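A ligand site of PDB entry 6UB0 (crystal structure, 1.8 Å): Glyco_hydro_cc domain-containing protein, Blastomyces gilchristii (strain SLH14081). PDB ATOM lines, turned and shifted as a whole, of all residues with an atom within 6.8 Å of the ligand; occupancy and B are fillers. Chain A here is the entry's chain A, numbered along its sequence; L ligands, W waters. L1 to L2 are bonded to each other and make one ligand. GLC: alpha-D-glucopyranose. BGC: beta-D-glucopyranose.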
ATOM      1  N   TYR A   9      -7.203 -28.349   5.703  1.00  0.00           N
ATOM      2  CA  TYR A   9      -8.114 -28.432   6.881  1.00  0.00           C
ATOM      3  C   TYR A   9      -9.129 -27.310   6.919  1.00  0.00           C
ATOM      4  O   TYR A   9      -9.008 -26.307   6.243  1.00  0.00           O
ATOM      5  CB  TYR A   9      -7.342 -28.305   8.186  1.00  0.00           C
ATOM      6  CG  TYR A   9      -6.675 -26.981   8.445  1.00  0.00           C
ATOM      7  CD1 TYR A   9      -5.453 -26.636   7.862  1.00  0.00           C
ATOM      8  CD2 TYR A   9      -7.280 -26.022   9.238  1.00  0.00           C
ATOM      9  CE1 TYR A   9      -4.819 -25.455   8.161  1.00  0.00           C
ATOM     10  CE2 TYR A   9      -6.663 -24.821   9.513  1.00  0.00           C
ATOM     11  CZ  TYR A   9      -5.454 -24.513   8.940  1.00  0.00           C
ATOM     12  OH  TYR A   9      -4.887 -23.327   9.271  1.00  0.00           O
ATOM     13  N   ASN A  10     -10.154 -27.527   7.717  1.00  0.00           N
ATOM     14  CA  ASN A  10     -11.082 -26.467   8.169  1.00  0.00           C
ATOM     15  C   ASN A  10     -10.880 -26.214   9.682  1.00  0.00           C
ATOM     16  O   ASN A  10     -10.658 -25.039  10.089  1.00  0.00           O
ATOM     17  CB  ASN A  10     -12.521 -26.843   7.801  1.00  0.00           C
ATOM     18  CG  ASN A  10     -12.864 -26.750   6.323  1.00  0.00           C
ATOM     19  OD1 ASN A  10     -13.917 -27.236   5.935  1.00  0.00           O
ATOM     20  ND2 ASN A  10     -12.042 -26.101   5.508  1.00  0.00           N
ATOM     21  N   TYR A  27      -3.086 -25.681   4.483  1.00  0.00           N
ATOM     22  CA  TYR A  27      -3.941 -24.588   3.983  1.00  0.00           C
ATOM     23  C   TYR A  27      -5.349 -24.980   4.370  1.00  0.00           C
ATOM     24  O   TYR A  27      -5.561 -26.137   4.698  1.00  0.00           O
ATOM     25  CB  TYR A  27      -3.667 -24.325   2.500  1.00  0.00           C
ATOM     26  CG  TYR A  27      -4.498 -25.105   1.515  1.00  0.00           C
ATOM     27  CD1 TYR A  27      -4.256 -26.462   1.326  1.00  0.00           C
ATOM     28  CD2 TYR A  27      -5.515 -24.509   0.778  1.00  0.00           C
ATOM     29  CE1 TYR A  27      -5.039 -27.205   0.446  1.00  0.00           C
ATOM     30  CE2 TYR A  27      -6.235 -25.210  -0.169  1.00  0.00           C
ATOM     31  CZ  TYR A  27      -6.025 -26.567  -0.317  1.00  0.00           C
ATOM     32  OH  TYR A  27      -6.781 -27.351  -1.168  1.00  0.00           O
ATOM     33  N   ASN A  28      -6.230 -24.020   4.289  1.00  0.00           N
ATOM     34  CA  ASN A  28      -7.621 -24.139   4.744  1.00  0.00           C
ATOM     35  C   ASN A  28      -8.572 -23.406   3.819  1.00  0.00           C
ATOM     36  O   ASN A  28      -9.666 -23.052   4.287  1.00  0.00           O
ATOM     37  CB  ASN A  28      -7.756 -23.577   6.143  1.00  0.00           C
ATOM     38  CG  ASN A  28      -7.452 -22.102   6.310  1.00  0.00           C
ATOM     39  OD1 ASN A  28      -6.914 -21.424   5.425  1.00  0.00           O
ATOM     40  ND2 ASN A  28      -7.838 -21.613   7.463  1.00  0.00           N
ATOM     41  N   TRP A  29      -8.183 -23.215   2.553  1.00  0.00           N
ATOM     42  CA  TRP A  29      -9.037 -22.541   1.542  1.00  0.00           C
ATOM     43  C   TRP A  29      -9.412 -21.125   1.995  1.00  0.00           C
ATOM     44  O   TRP A  29     -10.393 -20.583   1.425  1.00  0.00           O
ATOM     45  CB  TRP A  29     -10.315 -23.353   1.332  1.00  0.00           C
ATOM     46  CG  TRP A  29     -10.142 -24.687   0.698  1.00  0.00           C
ATOM     47  CD1 TRP A  29     -10.106 -24.937  -0.637  1.00  0.00           C
ATOM     48  CD2 TRP A  29      -9.990 -25.965   1.358  1.00  0.00           C
ATOM     49  NE1 TRP A  29      -9.936 -26.265  -0.857  1.00  0.00           N
ATOM     50  CE2 TRP A  29      -9.870 -26.923   0.338  1.00  0.00           C
ATOM     51  CE3 TRP A  29      -9.945 -26.376   2.680  1.00  0.00           C
ATOM     52  CZ2 TRP A  29      -9.670 -28.285   0.583  1.00  0.00           C
ATOM     53  CZ3 TRP A  29      -9.790 -27.739   2.937  1.00  0.00           C
ATOM     54  CH2 TRP A  29      -9.708 -28.671   1.911  1.00  0.00           C
ATOM     55  N   GLU A  30      -8.700 -20.551   2.974  1.00  0.00           N
ATOM     56  CA  GLU A  30      -8.991 -19.213   3.485  1.00  0.00           C
ATOM     57  C   GLU A  30      -7.715 -18.407   3.339  1.00  0.00           C
ATOM     58  O   GLU A  30      -6.634 -18.980   3.131  1.00  0.00           O
ATOM     59  CB  GLU A  30      -9.381 -19.210   4.966  1.00  0.00           C
ATOM     60  CG  GLU A  30     -10.682 -19.920   5.255  1.00  0.00           C
ATOM     61  CD  GLU A  30     -11.848 -19.224   4.610  1.00  0.00           C
ATOM     62  OE1 GLU A  30     -11.768 -17.989   4.384  1.00  0.00           O
ATOM     63  OE2 GLU A  30     -12.817 -19.949   4.304  1.00  0.00           O
ATOM     64  N   TRP A  47      -9.298 -17.073  -2.390  1.00  0.00           N
ATOM     65  CA  TRP A  47     -10.281 -18.118  -2.807  1.00  0.00           C
ATOM     66  C   TRP A  47     -10.994 -17.689  -4.090  1.00  0.00           C
ATOM     67  O   TRP A  47     -11.306 -18.555  -4.904  1.00  0.00           O
ATOM     68  CB  TRP A  47     -11.253 -18.327  -1.657  1.00  0.00           C
ATOM     69  CG  TRP A  47     -12.229 -19.420  -1.895  1.00  0.00           C
ATOM     70  CD1 TRP A  47     -12.093 -20.726  -1.540  1.00  0.00           C
ATOM     71  CD2 TRP A  47     -13.469 -19.304  -2.603  1.00  0.00           C
ATOM     72  NE1 TRP A  47     -13.219 -21.420  -1.894  1.00  0.00           N
ATOM     73  CE2 TRP A  47     -14.057 -20.582  -2.585  1.00  0.00           C
ATOM     74  CE3 TRP A  47     -14.162 -18.244  -3.218  1.00  0.00           C
ATOM     75  CZ2 TRP A  47     -15.307 -20.826  -3.170  1.00  0.00           C
ATOM     76  CZ3 TRP A  47     -15.392 -18.490  -3.794  1.00  0.00           C
ATOM     77  CH2 TRP A  47     -15.950 -19.764  -3.775  1.00  0.00           C
ATOM     78  N   ARG A  50     -14.810 -12.800  -3.296  1.00  0.00           N
ATOM     79  CA  ARG A  50     -15.305 -12.527  -1.917  1.00  0.00           C
ATOM     80  C   ARG A  50     -14.122 -12.147  -1.020  1.00  0.00           C
ATOM     81  O   ARG A  50     -14.370 -11.602   0.039  1.00  0.00           O
ATOM     82  CB  ARG A  50     -16.047 -13.722  -1.326  1.00  0.00           C
ATOM     83  CG  ARG A  50     -15.181 -14.921  -0.996  1.00  0.00           C
ATOM     84  CD  ARG A  50     -16.101 -16.016  -0.501  1.00  0.00           C
ATOM     85  NE  ARG A  50     -15.480 -17.249  -0.051  1.00  0.00           N
ATOM     86  CZ  ARG A  50     -16.000 -18.475  -0.238  1.00  0.00           C
ATOM     87  NH1 ARG A  50     -17.120 -18.633  -0.935  1.00  0.00           N
ATOM     88  NH2 ARG A  50     -15.359 -19.538   0.210  1.00  0.00           N
ATOM     89  N   ASN A  74     -10.000 -20.734  -5.874  1.00  0.00           N
ATOM     90  CA  ASN A  74     -10.447 -22.156  -5.756  1.00  0.00           C
ATOM     91  C   ASN A  74     -11.454 -22.521  -6.846  1.00  0.00           C
ATOM     92  O   ASN A  74     -12.641 -22.221  -6.669  1.00  0.00           O
ATOM     93  CB  ASN A  74     -11.061 -22.409  -4.401  1.00  0.00           C
ATOM     94  CG  ASN A  74     -11.092 -23.892  -4.129  1.00  0.00           C
ATOM     95  OD1 ASN A  74     -10.062 -24.536  -4.107  1.00  0.00           O
ATOM     96  ND2 ASN A  74     -12.293 -24.428  -4.017  1.00  0.00           N
ATOM     97  N   GLU A  75     -11.042 -23.326  -7.801  1.00  0.00           N
ATOM     98  CA  GLU A  75     -12.027 -23.906  -8.794  1.00  0.00           C
ATOM     99  C   GLU A  75     -12.828 -22.770  -9.434  1.00  0.00           C
ATOM    100  O   GLU A  75     -14.073 -22.713  -9.382  1.00  0.00           O
ATOM    101  CB  GLU A  75     -12.897 -24.992  -8.169  1.00  0.00           C
ATOM    102  CG  GLU A  75     -12.135 -26.299  -7.936  1.00  0.00           C
ATOM    103  CD  GLU A  75     -12.961 -27.483  -7.523  1.00  0.00           C
ATOM    104  OE1 GLU A  75     -14.211 -27.338  -7.506  1.00  0.00           O
ATOM    105  OE2 GLU A  75     -12.318 -28.570  -7.329  1.00  0.00           O
ATOM    106  N   ILE A  78     -15.744 -23.905 -11.670  1.00  0.00           N
ATOM    107  CA  ILE A  78     -16.971 -24.546 -11.086  1.00  0.00           C
ATOM    108  C   ILE A  78     -17.887 -23.454 -10.537  1.00  0.00           C
ATOM    109  O   ILE A  78     -17.434 -22.603  -9.806  1.00  0.00           O
ATOM    110  CB  ILE A  78     -16.570 -25.595 -10.016  1.00  0.00           C
ATOM    111  CG1 ILE A  78     -15.734 -26.723 -10.629  1.00  0.00           C
ATOM    112  CG2 ILE A  78     -17.790 -26.099  -9.238  1.00  0.00           C
ATOM    113  CD1 ILE A  78     -16.487 -27.753 -11.472  1.00  0.00           C
ATOM    114  N   SER A  80     -20.259 -23.069  -8.449  1.00  0.00           N
ATOM    115  CA  SER A  80     -20.533 -22.936  -6.988  1.00  0.00           C
ATOM    116  C   SER A  80     -19.222 -22.760  -6.218  1.00  0.00           C
ATOM    117  O   SER A  80     -19.303 -22.580  -5.003  1.00  0.00           O
ATOM    118  CB  SER A  80     -21.264 -24.102  -6.472  1.00  0.00           C
ATOM    119  OG  SER A  80     -20.446 -25.229  -6.577  1.00  0.00           O
ATOM    120  N   GLN A  81     -18.085 -22.772  -6.905  1.00  0.00           N
ATOM    121  CA  GLN A  81     -16.797 -22.366  -6.284  1.00  0.00           C
ATOM    122  C   GLN A  81     -16.489 -20.944  -6.732  1.00  0.00           C
ATOM    123  O   GLN A  81     -17.402 -20.088  -6.707  1.00  0.00           O
ATOM    124  CB  GLN A  81     -15.735 -23.393  -6.627  1.00  0.00           C
ATOM    125  CG  GLN A  81     -16.085 -24.779  -6.115  1.00  0.00           C
ATOM    126  CD  GLN A  81     -16.184 -24.792  -4.609  1.00  0.00           C
ATOM    127  OE1 GLN A  81     -15.464 -24.084  -3.913  1.00  0.00           O
ATOM    128  NE2 GLN A  81     -17.101 -25.585  -4.072  1.00  0.00           N
ATOM    129  N   ALA A  82     -15.251 -20.651  -7.078  1.00  0.00           N
ATOM    130  CA  ALA A  82     -14.856 -19.260  -7.338  1.00  0.00           C
ATOM    131  C   ALA A  82     -15.776 -18.716  -8.413  1.00  0.00           C
ATOM    132  O   ALA A  82     -16.072 -17.529  -8.337  1.00  0.00           O
ATOM    133  CB  ALA A  82     -13.405 -19.144  -7.740  1.00  0.00           C
ATOM    134  N   HIS A 142      -6.731 -30.007  -8.879  1.00  0.00           N
ATOM    135  CA  HIS A 142      -7.511 -30.902  -8.012  1.00  0.00           C
ATOM    136  C   HIS A 142      -7.960 -32.147  -8.778  1.00  0.00           C
ATOM    137  O   HIS A 142      -8.384 -31.941  -9.905  1.00  0.00           O
ATOM    138  CB  HIS A 142      -8.802 -30.260  -7.633  1.00  0.00           C
ATOM    139  CG  HIS A 142      -8.685 -29.093  -6.737  1.00  0.00           C
ATOM    140  ND1 HIS A 142      -9.761 -28.356  -6.439  1.00  0.00           N
ATOM    141  CD2 HIS A 142      -7.626 -28.545  -6.114  1.00  0.00           C
ATOM    142  CE1 HIS A 142      -9.425 -27.418  -5.591  1.00  0.00           C
ATOM    143  NE2 HIS A 142      -8.109 -27.481  -5.373  1.00  0.00           N
ATOM    144  N   HIS A 144     -10.737 -35.469  -8.033  1.00  0.00           N
ATOM    145  CA  HIS A 144     -11.681 -36.306  -7.248  1.00  0.00           C
ATOM    146  C   HIS A 144     -12.257 -37.359  -8.193  1.00  0.00           C
ATOM    147  O   HIS A 144     -12.569 -37.042  -9.337  1.00  0.00           O
ATOM    148  CB  HIS A 144     -12.823 -35.515  -6.639  1.00  0.00           C
ATOM    149  CG  HIS A 144     -12.395 -34.445  -5.683  1.00  0.00           C
ATOM    150  ND1 HIS A 144     -12.744 -34.477  -4.331  1.00  0.00           N
ATOM    151  CD2 HIS A 144     -11.688 -33.312  -5.874  1.00  0.00           C
ATOM    152  CE1 HIS A 144     -12.254 -33.415  -3.736  1.00  0.00           C
ATOM    153  NE2 HIS A 144     -11.593 -32.701  -4.648  1.00  0.00           N
ATOM    154  N   GLU A 176      -5.701 -30.714  -3.974  1.00  0.00           N
ATOM    155  CA  GLU A 176      -6.779 -31.630  -3.564  1.00  0.00           C
ATOM    156  C   GLU A 176      -6.645 -32.903  -4.402  1.00  0.00           C
ATOM    157  O   GLU A 176      -6.700 -32.813  -5.613  1.00  0.00           O
ATOM    158  CB  GLU A 176      -8.185 -31.129  -3.844  1.00  0.00           C
ATOM    159  CG  GLU A 176      -8.667 -29.970  -3.009  1.00  0.00           C
ATOM    160  CD  GLU A 176     -10.068 -29.482  -3.293  1.00  0.00           C
ATOM    161  OE1 GLU A 176     -10.792 -30.157  -4.051  1.00  0.00           O
ATOM    162  OE2 GLU A 176     -10.416 -28.386  -2.828  1.00  0.00           O
ATOM    163  N   GLU A 178      -8.704 -36.994  -4.041  1.00  0.00           N
ATOM    164  CA  GLU A 178      -9.575 -37.848  -3.214  1.00  0.00           C
ATOM    165  C   GLU A 178      -9.939 -39.084  -4.027  1.00  0.00           C
ATOM    166  O   GLU A 178     -10.606 -38.904  -5.049  1.00  0.00           O
ATOM    167  CB  GLU A 178     -10.800 -37.037  -2.784  1.00  0.00           C
ATOM    168  CG  GLU A 178     -11.841 -37.860  -2.099  1.00  0.00           C
ATOM    169  CD  GLU A 178     -13.121 -37.150  -1.730  1.00  0.00           C
ATOM    170  OE1 GLU A 178     -13.584 -36.267  -2.521  1.00  0.00           O
ATOM    171  OE2 GLU A 178     -13.653 -37.515  -0.647  1.00  0.00           O
ATOM    172  N   PHE A 209      -7.513 -34.934   0.190  1.00  0.00           N
ATOM    173  CA  PHE A 209      -8.726 -34.176   0.542  1.00  0.00           C
ATOM    174  C   PHE A 209      -9.561 -34.992   1.538  1.00  0.00           C
ATOM    175  O   PHE A 209     -10.153 -35.956   1.152  1.00  0.00           O
ATOM    176  CB  PHE A 209      -9.522 -33.855  -0.737  1.00  0.00           C
ATOM    177  CG  PHE A 209     -10.795 -33.122  -0.492  1.00  0.00           C
ATOM    178  CD1 PHE A 209     -10.853 -31.737  -0.396  1.00  0.00           C
ATOM    179  CD2 PHE A 209     -11.997 -33.830  -0.369  1.00  0.00           C
ATOM    180  CE1 PHE A 209     -12.047 -31.076  -0.208  1.00  0.00           C
ATOM    181  CE2 PHE A 209     -13.191 -33.156  -0.154  1.00  0.00           C
ATOM    182  CZ  PHE A 209     -13.227 -31.789  -0.091  1.00  0.00           C
ATOM    183  N   PHE A 210      -9.664 -34.606   2.814  1.00  0.00           N
ATOM    184  CA  PHE A 210      -8.856 -33.615   3.516  1.00  0.00           C
ATOM    185  C   PHE A 210      -8.826 -33.990   5.011  1.00  0.00           C
ATOM    186  O   PHE A 210      -9.511 -34.975   5.410  1.00  0.00           O
ATOM    187  CB  PHE A 210      -9.415 -32.210   3.359  1.00  0.00           C
ATOM    188  CG  PHE A 210     -10.830 -31.879   3.855  1.00  0.00           C
ATOM    189  CD1 PHE A 210     -11.939 -32.583   3.446  1.00  0.00           C
ATOM    190  CD2 PHE A 210     -10.992 -30.812   4.714  1.00  0.00           C
ATOM    191  CE1 PHE A 210     -13.188 -32.225   3.904  1.00  0.00           C
ATOM    192  CE2 PHE A 210     -12.256 -30.451   5.171  1.00  0.00           C
ATOM    193  CZ  PHE A 210     -13.336 -31.163   4.750  1.00  0.00           C
HETATM  194  C1  GLC L   1     -13.866 -29.403  -4.345  1.00  0.00           C
HETATM  195  C2  GLC L   1     -14.001 -28.013  -3.704  1.00  0.00           C
HETATM  196  C3  GLC L   1     -14.744 -28.092  -2.366  1.00  0.00           C
HETATM  197  C4  GLC L   1     -16.069 -28.874  -2.562  1.00  0.00           C
HETATM  198  C5  GLC L   1     -15.857 -30.186  -3.282  1.00  0.00           C
HETATM  199  C6  GLC L   1     -17.122 -31.026  -3.531  1.00  0.00           C
HETATM  200  O1  GLC L   1     -13.171 -30.351  -3.517  1.00  0.00           O
HETATM  201  O2  GLC L   1     -12.771 -27.299  -3.453  1.00  0.00           O
HETATM  202  O3  GLC L   1     -14.956 -26.761  -1.885  1.00  0.00           O
HETATM  203  O4  GLC L   1     -16.561 -29.223  -1.315  1.00  0.00           O
HETATM  204  O5  GLC L   1     -15.228 -29.880  -4.530  1.00  0.00           O
HETATM  205  O6  GLC L   1     -18.157 -30.097  -3.730  1.00  0.00           O
HETATM  206  C2  BGC L   2     -14.719 -25.037  -0.277  1.00  0.00           C
HETATM  207  C3  BGC L   2     -13.974 -24.512   0.912  1.00  0.00           C
HETATM  208  C4  BGC L   2     -14.023 -25.599   1.962  1.00  0.00           C
HETATM  209  C5  BGC L   2     -13.451 -26.922   1.392  1.00  0.00           C
HETATM  210  C6  BGC L   2     -13.494 -28.202   2.234  1.00  0.00           C
HETATM  211  C1  BGC L   2     -14.192 -26.370  -0.755  1.00  0.00           C
HETATM  212  O2  BGC L   2     -14.518 -24.065  -1.302  1.00  0.00           O
HETATM  213  O3  BGC L   2     -14.438 -23.204   1.361  1.00  0.00           O
HETATM  214  O4  BGC L   2     -13.278 -25.037   3.045  1.00  0.00           O
HETATM  215  O5  BGC L   2     -14.190 -27.380   0.251  1.00  0.00           O
HETATM  216  O6  BGC L   2     -14.842 -28.329   2.758  1.00  0.00           O
HETATM  217  O   HOH W   1     -14.033 -22.812   4.676  1.00  0.00           O
HETATM  218  O   HOH W   2     -16.398 -28.623  -6.624  1.00  0.00           O
HETATM  219  O   HOH W   3     -12.906 -21.059   1.978  1.00  0.00           O
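Water W3 lies within hydrogen-bond range of the side-chain carboxylate of Glu 30 (2.6 Å), the backbone carbonyl oxygen of Trp 29 (2.6 Å), an oxygen (O3) of BGC L2 (2.7 Å) and the guanidinium group of Arg 50 (3.4 Å). Water W2 bridges OE1 of Glu 75 and O5 of GLC L1. Water W1 lies within hydrogen-bond range of an oxygen (O4) of BGC L2 (2.9 Å) and the side-chain carboxylate of Glu 30 (3.1 Å).
NE2 of His 144 sits at hydrogen-bond distance from OE1 of Glu 176 (2.7 Å). ND2 of Asn 74 is in hydrogen-bond range of OE1 of Gln 81 (3.2 Å). The backbone carbonyl oxygen (O) of Trp 47 lies within hydrogen-bond range of the backbone NH (N) of Asn 74 (2.7 Å). The backbone carbonyl oxygen of Asn 74 is in hydrogen-bond range of the backbone NH of Ala 82 (3.1 Å). OE1 of Glu 178 sits at hydrogen-bond distance from ND1 of His 144 (2.7 Å). OE2 of Glu 75 is in hydrogen-bond range of ND1 of His 142. N of Ala 82 is in hydrogen-bond range of O of Glu 75 (3.3 Å). The side-chain hydroxyl of Tyr 27 is in hydrogen-bond range of the indole nitrogen of Trp 29.
CD2 of Trp 29 touches C5 of BGC L2, at 3.6 Å. NH2 of Arg 50 touches O3 of BGC L2 (3.95 Å). Glu 75 touches the ligand. CE1 of His 142 touches O2 of GLC L1 (3.97 Å). CE1 of Phe 209 touches O1 of GLC L1, 3.6 Å away. CZ of Phe 210 touches O6 of BGC L2 (3.8 Å). Hydrophobic or aromatic side chains within 4 Å of the ligand: Trp 29, Trp 47, His 142, His 144, Phe 209 and Phe 210. Of the 20 residues printed, 12 come within 4 Å of the ligand. Along chain A the residues within 4 Å of the ligand span positions 10 to 210. The nearest printed residue that does not touch the ligand is Asn 28 (4.3 Å).
The side-chain carboxylate of Glu 176 lies within hydrogen-bond range of an oxygen (O1) of GLC L1, at 2.4 Å. O2 of BGC L2 is in hydrogen-bond range of OE1 of Gln 81 (2.8 Å). The side-chain amide nitrogen of Asn 10 lies within hydrogen-bond range of an oxygen (O4) of BGC L2 (3.0 Å). The side-chain amide nitrogen (ND2) of Asn 74 sits at hydrogen-bond distance from an oxygen (O2) of GLC L1 (3.0 Å). NE1 of Trp 47 lies within hydrogen-bond range of O2 of BGC L2. NE2 of His 144 sits at hydrogen-bond distance from O1 of GLC L1 (3.0 Å).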
